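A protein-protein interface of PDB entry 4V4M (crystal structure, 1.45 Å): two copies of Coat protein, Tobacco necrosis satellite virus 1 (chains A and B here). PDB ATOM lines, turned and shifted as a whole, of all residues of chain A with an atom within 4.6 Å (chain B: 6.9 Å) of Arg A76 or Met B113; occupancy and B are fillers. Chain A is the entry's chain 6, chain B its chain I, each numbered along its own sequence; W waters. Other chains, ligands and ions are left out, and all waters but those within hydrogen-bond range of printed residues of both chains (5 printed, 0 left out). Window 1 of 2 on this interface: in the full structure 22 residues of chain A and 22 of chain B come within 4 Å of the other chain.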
ATOM      1  N   ILE A  33     -28.809  36.204  21.847  1.00  0.00           N
ATOM      2  CA  ILE A  33     -27.941  35.504  20.892  1.00  0.00           C
ATOM      3  C   ILE A  33     -26.521  35.424  21.454  1.00  0.00           C
ATOM      4  O   ILE A  33     -26.085  36.335  22.150  1.00  0.00           O
ATOM      5  CB  ILE A  33     -27.962  36.189  19.490  1.00  0.00           C
ATOM      6  CG1 ILE A  33     -27.457  35.237  18.406  1.00  0.00           C
ATOM      7  CG2 ILE A  33     -27.167  37.508  19.508  1.00  0.00           C
ATOM      8  CD1 ILE A  33     -27.966  35.621  17.012  1.00  0.00           C
ATOM      9  N   HIS A  74     -31.829  27.405  20.433  1.00  0.00           N
ATOM     10  CA  HIS A  74     -31.250  27.011  19.145  1.00  0.00           C
ATOM     11  C   HIS A  74     -29.760  26.857  19.411  1.00  0.00           C
ATOM     12  O   HIS A  74     -29.126  27.802  19.911  1.00  0.00           O
ATOM     13  CB  HIS A  74     -31.491  28.150  18.150  1.00  0.00           C
ATOM     14  CG  HIS A  74     -31.277  27.806  16.701  1.00  0.00           C
ATOM     15  ND1 HIS A  74     -30.543  26.722  16.265  1.00  0.00           N
ATOM     16  CD2 HIS A  74     -31.688  28.452  15.580  1.00  0.00           C
ATOM     17  CE1 HIS A  74     -30.527  26.702  14.940  1.00  0.00           C
ATOM     18  NE2 HIS A  74     -31.216  27.741  14.500  1.00  0.00           N
ATOM     19  N   VAL A  75     -29.202  25.686  19.102  1.00  0.00           N
ATOM     20  CA  VAL A  75     -27.754  25.462  19.244  1.00  0.00           C
ATOM     21  C   VAL A  75     -27.146  25.039  17.917  1.00  0.00           C
ATOM     22  O   VAL A  75     -27.807  24.416  17.097  1.00  0.00           O
ATOM     23  CB  VAL A  75     -27.402  24.413  20.330  1.00  0.00           C
ATOM     24  CG1 VAL A  75     -27.827  24.902  21.719  1.00  0.00           C
ATOM     25  CG2 VAL A  75     -28.046  23.071  20.008  1.00  0.00           C
ATOM     26  N   ARG A  76     -25.880  25.377  17.721  1.00  0.00           N
ATOM     27  CA  ARG A  76     -25.192  25.096  16.457  1.00  0.00           C
ATOM     28  C   ARG A  76     -23.704  24.856  16.692  1.00  0.00           C
ATOM     29  O   ARG A  76     -23.072  25.548  17.498  1.00  0.00           O
ATOM     30  CB  ARG A  76     -25.350  26.277  15.502  1.00  0.00           C
ATOM     31  CG  ARG A  76     -24.583  26.162  14.194  1.00  0.00           C
ATOM     32  CD  ARG A  76     -24.768  27.457  13.425  1.00  0.00           C
ATOM     33  NE  ARG A  76     -24.471  27.364  11.997  1.00  0.00           N
ATOM     34  CZ  ARG A  76     -23.381  27.886  11.437  1.00  0.00           C
ATOM     35  NH1 ARG A  76     -22.474  28.503  12.196  1.00  0.00           N
ATOM     36  NH2 ARG A  76     -23.203  27.794  10.126  1.00  0.00           N
ATOM     37  N   GLY A  77     -23.157  23.890  15.968  1.00  0.00           N
ATOM     38  CA  GLY A  77     -21.746  23.553  16.049  1.00  0.00           C
ATOM     39  C   GLY A  77     -21.121  23.514  14.673  1.00  0.00           C
ATOM     40  O   GLY A  77     -21.762  23.076  13.700  1.00  0.00           O
ATOM     41  N   THR A  78     -19.874  23.992  14.595  1.00  0.00           N
ATOM     42  CA  THR A  78     -19.078  23.911  13.378  1.00  0.00           C
ATOM     43  C   THR A  78     -17.711  23.340  13.694  1.00  0.00           C
ATOM     44  O   THR A  78     -16.962  23.933  14.478  1.00  0.00           O
ATOM     45  CB  THR A  78     -18.855  25.297  12.742  1.00  0.00           C
ATOM     46  OG1 THR A  78     -20.117  25.899  12.439  1.00  0.00           O
ATOM     47  CG2 THR A  78     -18.066  25.164  11.460  1.00  0.00           C
ATOM     48  N   PHE A  88     -24.665  20.054  24.285  1.00  0.00           N
ATOM     49  CA  PHE A  88     -25.388  21.179  24.856  1.00  0.00           C
ATOM     50  C   PHE A  88     -26.414  20.616  25.826  1.00  0.00           C
ATOM     51  O   PHE A  88     -27.206  19.751  25.441  1.00  0.00           O
ATOM     52  CB  PHE A  88     -26.110  21.967  23.755  1.00  0.00           C
ATOM     53  CG  PHE A  88     -25.204  22.421  22.628  1.00  0.00           C
ATOM     54  CD1 PHE A  88     -25.020  21.627  21.519  1.00  0.00           C
ATOM     55  CD2 PHE A  88     -24.531  23.636  22.699  1.00  0.00           C
ATOM     56  CE1 PHE A  88     -24.164  22.048  20.464  1.00  0.00           C
ATOM     57  CE2 PHE A  88     -23.696  24.060  21.664  1.00  0.00           C
ATOM     58  CZ  PHE A  88     -23.522  23.268  20.546  1.00  0.00           C
ATOM     59  N   ILE A 143     -21.245  21.215   9.796  1.00  0.00           N
ATOM     60  CA  ILE A 143     -22.169  22.130  10.488  1.00  0.00           C
ATOM     61  C   ILE A 143     -23.470  21.414  10.870  1.00  0.00           C
ATOM     62  O   ILE A 143     -24.154  20.817  10.020  1.00  0.00           O
ATOM     63  CB  ILE A 143     -22.521  23.358   9.607  1.00  0.00           C
ATOM     64  CG1 ILE A 143     -21.244  24.065   9.136  1.00  0.00           C
ATOM     65  CG2 ILE A 143     -23.482  24.322  10.341  1.00  0.00           C
ATOM     66  CD1 ILE A 143     -21.487  25.051   8.027  1.00  0.00           C
ATOM     67  N   LYS A 144     -23.818  21.488  12.146  1.00  0.00           N
ATOM     68  CA  LYS A 144     -25.070  20.892  12.608  1.00  0.00           C
ATOM     69  C   LYS A 144     -25.772  21.839  13.565  1.00  0.00           C
ATOM     70  O   LYS A 144     -25.132  22.631  14.258  1.00  0.00           O
ATOM     71  CB  LYS A 144     -24.813  19.529  13.263  1.00  0.00           C
ATOM     72  CG  LYS A 144     -24.388  18.469  12.238  1.00  0.00           C
ATOM     73  CD  LYS A 144     -24.268  17.098  12.858  1.00  0.00           C
ATOM     74  CE  LYS A 144     -23.916  16.064  11.793  1.00  0.00           C
ATOM     75  NZ  LYS A 144     -23.828  14.708  12.420  1.00  0.00           N
ATOM     76  N   ASP A 145     -27.094  21.768  13.603  1.00  0.00           N
ATOM     77  CA  ASP A 145     -27.864  22.646  14.487  1.00  0.00           C
ATOM     78  C   ASP A 145     -29.114  21.934  14.974  1.00  0.00           C
ATOM     79  O   ASP A 145     -29.562  20.941  14.378  1.00  0.00           O
ATOM     80  CB  ASP A 145     -28.233  23.977  13.791  1.00  0.00           C
ATOM     81  CG  ASP A 145     -29.432  23.844  12.853  1.00  0.00           C
ATOM     82  OD1 ASP A 145     -29.353  23.056  11.886  1.00  0.00           O
ATOM     83  OD2 ASP A 145     -30.462  24.534  13.068  1.00  0.00           O
ATOM     84  N   LEU A 184     -16.223  25.904  16.730  1.00  0.00           N
ATOM     85  CA  LEU A 184     -17.032  27.034  17.215  1.00  0.00           C
ATOM     86  C   LEU A 184     -18.507  26.684  17.329  1.00  0.00           C
ATOM     87  O   LEU A 184     -19.058  25.946  16.496  1.00  0.00           O
ATOM     88  CB  LEU A 184     -16.873  28.241  16.286  1.00  0.00           C
ATOM     89  CG  LEU A 184     -15.499  28.913  16.267  1.00  0.00           C
ATOM     90  CD1 LEU A 184     -15.508  30.071  15.245  1.00  0.00           C
ATOM     91  CD2 LEU A 184     -15.096  29.402  17.638  1.00  0.00           C
ATOM     92  N   TRP A 185     -19.147  27.200  18.371  1.00  0.00           N
ATOM     93  CA  TRP A 185     -20.591  27.014  18.511  1.00  0.00           C
ATOM     94  C   TRP A 185     -21.329  28.335  18.693  1.00  0.00           C
ATOM     95  O   TRP A 185     -20.755  29.334  19.175  1.00  0.00           O
ATOM     96  CB  TRP A 185     -20.927  26.049  19.665  1.00  0.00           C
ATOM     97  CG  TRP A 185     -20.490  26.486  21.029  1.00  0.00           C
ATOM     98  CD1 TRP A 185     -19.290  26.218  21.629  1.00  0.00           C
ATOM     99  CD2 TRP A 185     -21.229  27.284  21.959  1.00  0.00           C
ATOM    100  NE1 TRP A 185     -19.234  26.797  22.867  1.00  0.00           N
ATOM    101  CE2 TRP A 185     -20.416  27.447  23.107  1.00  0.00           C
ATOM    102  CE3 TRP A 185     -22.503  27.879  21.939  1.00  0.00           C
ATOM    103  CZ2 TRP A 185     -20.829  28.177  24.227  1.00  0.00           C
ATOM    104  CZ3 TRP A 185     -22.917  28.599  23.064  1.00  0.00           C
ATOM    105  CH2 TRP A 185     -22.077  28.748  24.186  1.00  0.00           C
ATOM    106  N   ASP A 186     -22.607  28.320  18.313  1.00  0.00           N
ATOM    107  CA  ASP A 186     -23.487  29.480  18.414  1.00  0.00           C
ATOM    108  C   ASP A 186     -24.747  29.039  19.125  1.00  0.00           C
ATOM    109  O   ASP A 186     -25.133  27.874  19.031  1.00  0.00           O
ATOM    110  CB  ASP A 186     -23.861  29.997  17.006  1.00  0.00           C
ATOM    111  CG  ASP A 186     -22.669  30.059  16.074  1.00  0.00           C
ATOM    112  OD1 ASP A 186     -21.746  30.861  16.334  1.00  0.00           O
ATOM    113  OD2 ASP A 186     -22.641  29.279  15.098  1.00  0.00           O
ATOM    114  N   SER A 187     -25.401  29.963  19.813  1.00  0.00           N
ATOM    115  CA  SER A 187     -26.701  29.671  20.392  1.00  0.00           C
ATOM    116  C   SER A 187     -27.587  30.909  20.359  1.00  0.00           C
ATOM    117  O   SER A 187     -27.103  32.051  20.259  1.00  0.00           O
ATOM    118  CB  SER A 187     -26.573  29.144  21.832  1.00  0.00           C
ATOM    119  OG  SER A 187     -26.198  30.178  22.725  1.00  0.00           O
ATOM    120  N   SER A 188     -28.892  30.690  20.457  1.00  0.00           N
ATOM    121  CA  SER A 188     -29.841  31.772  20.684  1.00  0.00           C
ATOM    122  C   SER A 188     -30.993  31.217  21.512  1.00  0.00           C
ATOM    123  O   SER A 188     -31.199  29.993  21.579  1.00  0.00           O
ATOM    124  CB  SER A 188     -30.355  32.377  19.363  1.00  0.00           C
ATOM    125  OG  SER A 188     -31.075  31.400  18.629  1.00  0.00           O
ATOM    126  N   SER B  83     -18.488  25.604   3.258  1.00  0.00           N
ATOM    127  CA  SER B  83     -19.684  24.994   3.809  1.00  0.00           C
ATOM    128  C   SER B  83     -20.442  26.087   4.545  1.00  0.00           C
ATOM    129  O   SER B  83     -19.833  26.974   5.156  1.00  0.00           O
ATOM    130  CB  SER B  83     -19.307  23.865   4.764  1.00  0.00           C
ATOM    131  OG  SER B  83     -18.567  22.871   4.061  1.00  0.00           O
ATOM    132  N   GLN B  84     -21.767  26.067   4.462  1.00  0.00           N
ATOM    133  CA  GLN B  84     -22.512  27.203   4.981  1.00  0.00           C
ATOM    134  C   GLN B  84     -23.966  26.872   5.240  1.00  0.00           C
ATOM    135  O   GLN B  84     -24.468  25.818   4.834  1.00  0.00           O
ATOM    136  CB  GLN B  84     -22.433  28.368   3.989  1.00  0.00           C
ATOM    137  CG  GLN B  84     -22.988  28.015   2.599  1.00  0.00           C
ATOM    138  CD  GLN B  84     -22.686  29.092   1.581  1.00  0.00           C
ATOM    139  OE1 GLN B  84     -23.480  30.018   1.384  1.00  0.00           O
ATOM    140  NE2 GLN B  84     -21.513  28.994   0.946  1.00  0.00           N
ATOM    141  N   THR B  85     -24.636  27.795   5.907  1.00  0.00           N
ATOM    142  CA  THR B  85     -26.002  27.624   6.330  1.00  0.00           C
ATOM    143  C   THR B  85     -26.926  28.604   5.617  1.00  0.00           C
ATOM    144  O   THR B  85     -26.608  29.799   5.486  1.00  0.00           O
ATOM    145  CB  THR B  85     -26.108  27.876   7.833  1.00  0.00           C
ATOM    146  OG1 THR B  85     -25.400  26.847   8.531  1.00  0.00           O
ATOM    147  CG2 THR B  85     -27.582  27.873   8.257  1.00  0.00           C
ATOM    148  N   ARG B  87     -30.995  29.841   5.793  1.00  0.00           N
ATOM    149  CA  ARG B  87     -32.244  29.824   6.549  1.00  0.00           C
ATOM    150  C   ARG B  87     -33.336  30.470   5.714  1.00  0.00           C
ATOM    151  O   ARG B  87     -33.112  31.497   5.049  1.00  0.00           O
ATOM    152  CB  ARG B  87     -32.083  30.538   7.900  1.00  0.00           C
ATOM    153  CG  ARG B  87     -33.338  30.574   8.773  1.00  0.00           C
ATOM    154  CD  ARG B  87     -33.047  31.267  10.110  1.00  0.00           C
ATOM    155  NE  ARG B  87     -34.234  31.360  10.972  1.00  0.00           N
ATOM    156  CZ  ARG B  87     -34.255  32.038  12.120  1.00  0.00           C
ATOM    157  NH1 ARG B  87     -33.166  32.676  12.534  1.00  0.00           N
ATOM    158  NH2 ARG B  87     -35.356  32.098  12.861  1.00  0.00           N
ATOM    159  N   LEU B 107     -36.874  39.370  12.609  1.00  0.00           N
ATOM    160  CA  LEU B 107     -35.836  38.827  13.483  1.00  0.00           C
ATOM    161  C   LEU B 107     -35.291  39.859  14.462  1.00  0.00           C
ATOM    162  O   LEU B 107     -35.125  41.040  14.130  1.00  0.00           O
ATOM    163  CB  LEU B 107     -34.674  38.329  12.627  1.00  0.00           C
ATOM    164  CG  LEU B 107     -34.938  37.122  11.725  1.00  0.00           C
ATOM    165  CD1 LEU B 107     -33.657  36.763  10.950  1.00  0.00           C
ATOM    166  CD2 LEU B 107     -35.360  35.954  12.581  1.00  0.00           C
ATOM    167  N   THR B 109     -32.294  40.314  15.706  1.00  0.00           N
ATOM    168  CA  THR B 109     -31.094  40.886  15.066  1.00  0.00           C
ATOM    169  C   THR B 109     -30.938  40.258  13.685  1.00  0.00           C
ATOM    170  O   THR B 109     -31.484  39.182  13.411  1.00  0.00           O
ATOM    171  CB  THR B 109     -29.778  40.680  15.891  1.00  0.00           C
ATOM    172  OG1 THR B 109     -29.590  39.282  16.172  1.00  0.00           O
ATOM    173  CG2 THR B 109     -29.826  41.458  17.202  1.00  0.00           C
ATOM    174  N   ALA B 110     -30.229  40.950  12.804  1.00  0.00           N
ATOM    175  CA  ALA B 110     -30.056  40.470  11.438  1.00  0.00           C
ATOM    176  C   ALA B 110     -28.938  39.443  11.390  1.00  0.00           C
ATOM    177  O   ALA B 110     -27.832  39.696  10.902  1.00  0.00           O
ATOM    178  CB  ALA B 110     -29.785  41.633  10.481  1.00  0.00           C
ATOM    179  N   ASN B 111     -29.247  38.262  11.916  1.00  0.00           N
ATOM    180  CA  ASN B 111     -28.310  37.148  11.968  1.00  0.00           C
ATOM    181  C   ASN B 111     -29.092  35.860  11.798  1.00  0.00           C
ATOM    182  O   ASN B 111     -30.207  35.733  12.314  1.00  0.00           O
ATOM    183  CB  ASN B 111     -27.560  37.119  13.309  1.00  0.00           C
ATOM    184  CG  ASN B 111     -26.470  36.057  13.345  1.00  0.00           C
ATOM    185  OD1 ASN B 111     -26.735  34.895  13.641  1.00  0.00           O
ATOM    186  ND2 ASN B 111     -25.219  36.464  13.093  1.00  0.00           N
ATOM    187  N   PHE B 112     -28.503  34.916  11.078  1.00  0.00           N
ATOM    188  CA  PHE B 112     -29.187  33.670  10.753  1.00  0.00           C
ATOM    189  C   PHE B 112     -29.530  32.827  11.998  1.00  0.00           C
ATOM    190  O   PHE B 112     -30.385  31.957  11.916  1.00  0.00           O
ATOM    191  CB  PHE B 112     -28.369  32.863   9.744  1.00  0.00           C
ATOM    192  CG  PHE B 112     -27.193  32.161  10.356  1.00  0.00           C
ATOM    193  CD1 PHE B 112     -27.252  30.802  10.662  1.00  0.00           C
ATOM    194  CD2 PHE B 112     -26.046  32.859  10.653  1.00  0.00           C
ATOM    195  CE1 PHE B 112     -26.170  30.170  11.246  1.00  0.00           C
ATOM    196  CE2 PHE B 112     -24.965  32.223  11.259  1.00  0.00           C
ATOM    197  CZ  PHE B 112     -25.024  30.887  11.541  1.00  0.00           C
ATOM    198  N   MET B 113     -28.869  33.078  13.127  1.00  0.00           N
ATOM    199  CA  MET B 113     -29.220  32.403  14.397  1.00  0.00           C
ATOM    200  C   MET B 113     -30.280  33.119  15.250  1.00  0.00           C
ATOM    201  O   MET B 113     -30.724  32.582  16.266  1.00  0.00           O
ATOM    202  CB  MET B 113     -27.979  32.210  15.275  1.00  0.00           C
ATOM    203  CG  MET B 113     -27.029  31.118  14.818  1.00  0.00           C
ATOM    204  SD  MET B 113     -27.723  29.482  15.013  1.00  0.00           S
ATOM    205  CE  MET B 113     -27.787  29.332  16.805  1.00  0.00           C
ATOM    206  N   SER B 114     -30.663  34.332  14.867  1.00  0.00           N
ATOM    207  CA  SER B 114     -31.579  35.121  15.698  1.00  0.00           C
ATOM    208  C   SER B 114     -32.934  34.473  15.957  1.00  0.00           C
ATOM    209  O   SER B 114     -33.517  33.814  15.093  1.00  0.00           O
ATOM    210  CB  SER B 114     -31.800  36.514  15.084  1.00  0.00           C
ATOM    211  OG  SER B 114     -32.578  37.342  15.949  1.00  0.00           O
ATOM    212  N   GLN B 115     -33.448  34.737  17.147  1.00  0.00           N
ATOM    213  CA  GLN B 115     -34.841  34.474  17.464  1.00  0.00           C
ATOM    214  C   GLN B 115     -35.727  35.577  16.859  1.00  0.00           C
ATOM    215  O   GLN B 115     -35.219  36.578  16.318  1.00  0.00           O
ATOM    216  CB  GLN B 115     -35.014  34.383  18.981  1.00  0.00           C
ATOM    217  CG  GLN B 115     -34.152  33.305  19.607  1.00  0.00           C
ATOM    218  CD  GLN B 115     -34.744  31.920  19.472  1.00  0.00           C
ATOM    219  OE1 GLN B 115     -35.965  31.752  19.389  1.00  0.00           O
ATOM    220  NE2 GLN B 115     -33.880  30.909  19.454  1.00  0.00           N
ATOM    221  N   THR B 133     -33.937  25.540   8.254  1.00  0.00           N
ATOM    222  CA  THR B 133     -32.499  25.770   8.197  1.00  0.00           C
ATOM    223  C   THR B 133     -31.813  24.591   7.489  1.00  0.00           C
ATOM    224  O   THR B 133     -31.996  23.429   7.888  1.00  0.00           O
ATOM    225  CB  THR B 133     -31.910  25.969   9.620  1.00  0.00           C
ATOM    226  OG1 THR B 133     -32.298  27.252  10.146  1.00  0.00           O
ATOM    227  CG2 THR B 133     -30.383  25.863   9.609  1.00  0.00           C
ATOM    228  N   ASN B 135     -28.068  23.154   6.223  1.00  0.00           N
ATOM    229  CA  ASN B 135     -26.618  23.232   6.358  1.00  0.00           C
ATOM    230  C   ASN B 135     -25.986  22.456   5.216  1.00  0.00           C
ATOM    231  O   ASN B 135     -26.130  21.220   5.132  1.00  0.00           O
ATOM    232  CB  ASN B 135     -26.182  22.616   7.684  1.00  0.00           C
ATOM    233  CG  ASN B 135     -26.864  23.261   8.877  1.00  0.00           C
ATOM    234  OD1 ASN B 135     -27.360  22.574   9.780  1.00  0.00           O
ATOM    235  ND2 ASN B 135     -26.898  24.577   8.887  1.00  0.00           N
ATOM    236  N   ILE B 177     -31.788  34.197   5.035  1.00  0.00           N
ATOM    237  CA  ILE B 177     -30.603  34.694   5.728  1.00  0.00           C
ATOM    238  C   ILE B 177     -29.667  33.531   5.993  1.00  0.00           C
ATOM    239  O   ILE B 177     -30.116  32.391   6.232  1.00  0.00           O
ATOM    240  CB  ILE B 177     -30.989  35.446   7.032  1.00  0.00           C
ATOM    241  CG1 ILE B 177     -29.784  36.225   7.610  1.00  0.00           C
ATOM    242  CG2 ILE B 177     -31.619  34.486   8.034  1.00  0.00           C
ATOM    243  CD1 ILE B 177     -30.169  37.222   8.709  1.00  0.00           C
ATOM    244  N   GLY B 178     -28.363  33.789   5.947  1.00  0.00           N
ATOM    245  CA  GLY B 178     -27.406  32.718   6.166  1.00  0.00           C
ATOM    246  C   GLY B 178     -26.071  33.232   6.671  1.00  0.00           C
ATOM    247  O   GLY B 178     -25.963  34.393   7.068  1.00  0.00           O
ATOM    248  N   ASP B 179     -25.050  32.380   6.658  1.00  0.00           N
ATOM    249  CA  ASP B 179     -23.761  32.772   7.246  1.00  0.00           C
ATOM    250  C   ASP B 179     -22.646  33.007   6.226  1.00  0.00           C
ATOM    251  O   ASP B 179     -21.461  33.047   6.599  1.00  0.00           O
ATOM    252  CB  ASP B 179     -23.280  31.775   8.302  1.00  0.00           C
ATOM    253  CG  ASP B 179     -22.813  30.473   7.697  1.00  0.00           C
ATOM    254  OD1 ASP B 179     -21.915  29.824   8.283  1.00  0.00           O
ATOM    255  OD2 ASP B 179     -23.323  30.100   6.620  1.00  0.00           O
HETATM  256  O   HOH W   1     -20.740  30.577  10.558  1.00  0.00           O
HETATM  257  O   HOH W   2     -26.670  19.481   9.421  1.00  0.00           O
HETATM  258  O   HOH W   3     -26.748  25.902  11.345  1.00  0.00           O
HETATM  259  O   HOH W   4     -31.022  22.209  10.269  1.00  0.00           O
HETATM  260  O   HOH W   5     -28.545  27.437  12.386  1.00  0.00           O
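Water W4 bridges the side-chain carboxylate of Asp A145 (2.5 Å) and the backbone carbonyl oxygen of Thr B133 (2.8 Å).
Water W1 bridges OD1 of Asp B179 and NH1 of Arg A76.
Water W3 lies within hydrogen-bond range of NE of Arg A76 (2.8 Å), ND2 of Asn B135 (2.8 Å) and OG1 of Thr B85 (3.3 Å).
Water W2 bridges the backbone carbonyl oxygen of Ile A143 (2.9 Å) and the side-chain amide oxygen of Asn B135 (3.2 Å).
Water W5 bridges a ring nitrogen (NE2) of His A74 (3.4 Å) and the side-chain sulfur (SD) of Met B113 (3.4 Å).
The side-chain hydroxyl (OG) of Ser A188 lies within hydrogen-bond range of the side-chain amide nitrogen (NE2) of Gln B115 (3.0 Å).
OG of Ser A188 sits at hydrogen-bond distance from O of Met B113 (2.7 Å).
The side-chain carboxylate (OD1) of Asp B179 is in salt-bridge range of the guanidinium group (NH2) of Arg A76, at 3.0 Å.
NH2 of Arg A76 sits at hydrogen-bond distance from OG1 of Thr B85 (2.9 Å).
OD1 of Asn B135 lies close to OD1 of Asp A145.
Arg A76 touches just these residues of chain B: Thr B85 (2.9 Å), Phe B112 (3.4 Å), Met B113 (3.9 Å) and Asp B179 (3.0 Å).
Met B113 touches just these residues of chain A: Ile A33, His A74, Arg A76, Asp A186, Ser A187 and Ser A188.
Printed residues of chain B within 4 Å of Asp A145: Thr B133 (3.7 Å) and Asn B135 (2.9 Å).
Printed residues of chain B within 4 Å of Ser A188: Met B113 (2.7 Å) and Gln B115 (3.0 Å).
Of the printed residues of chain A, Asn B111 touches Ile A33.
Printed residues of chain B within 4 Å of His A74: Met B113 and Gln B115.
Trp A185 touches none of the printed residues of chain B.
The nearest residue of chain B that does not touch Arg A76 is Asn B135 (4.8 Å).
The nearest printed residue of chain B that does not touch Ile A33 is Thr B109 (4.1 Å).
Of the 17 printed residues of chain B, 11 touch a printed residue of chain A.
Hydrophobic or aromatic side chains of chain B within 4 Å of the printed part of chain A: Phe B112 and Met B113.
Of the 15 printed residues of chain A, 8 touch a printed residue of chain B.
Hydrophobic or aromatic side chains of chain A that line the printed part of chain B: Ile A33, His A74 and Ile A143.
Among the printed residues, Asp or Glu carboxylates within 4 Å of a Lys or Arg side-chain nitrogen of the other chain: Arg A76 with Asp B179.
No position is printed for both chains.
Asn B111 touches Ile A33 (OD1 to CD1, 3.7 Å).
N of Ser B114 touches CD1 of Ile A33, at 3.7 Å.
CE of Met B113 touches O of His A74, at 3.7 Å.
Gln B115 touches His A74.
NE of Arg A76 touches CE1 of Phe B112 (3.4 Å).
C of Ser B83 touches CD1 of Ile A143, at 3.8 Å.
Thr B85 touches Ile A143.
Thr B133 touches Asp A145.
Met B113 touches Asp A186.
Ser A187 touches Met B113 (CA to CE, 3.8 Å).
The backbone NH (N) of Thr B85 sits at hydrogen-bond distance from the side-chain carboxylate (OD2) of Asp B179 (2.7 Å).
The backbone carbonyl oxygen of Ser B114 lies within hydrogen-bond range of the guanidinium group of Arg B87, at 2.8 Å.
N of Thr B109 lies within hydrogen-bond range of OG of Ser B114 (3.0 Å).
The backbone NH of Met B113 is in hydrogen-bond range of the side-chain amide oxygen of Asn B111 (2.8 Å).
NH1 of Arg B87 lies within hydrogen-bond range of O of Phe B112 (2.9 Å).
ND2 of Asn B135 lies within hydrogen-bond range of OG1 of Thr B85, 2.7 Å away.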
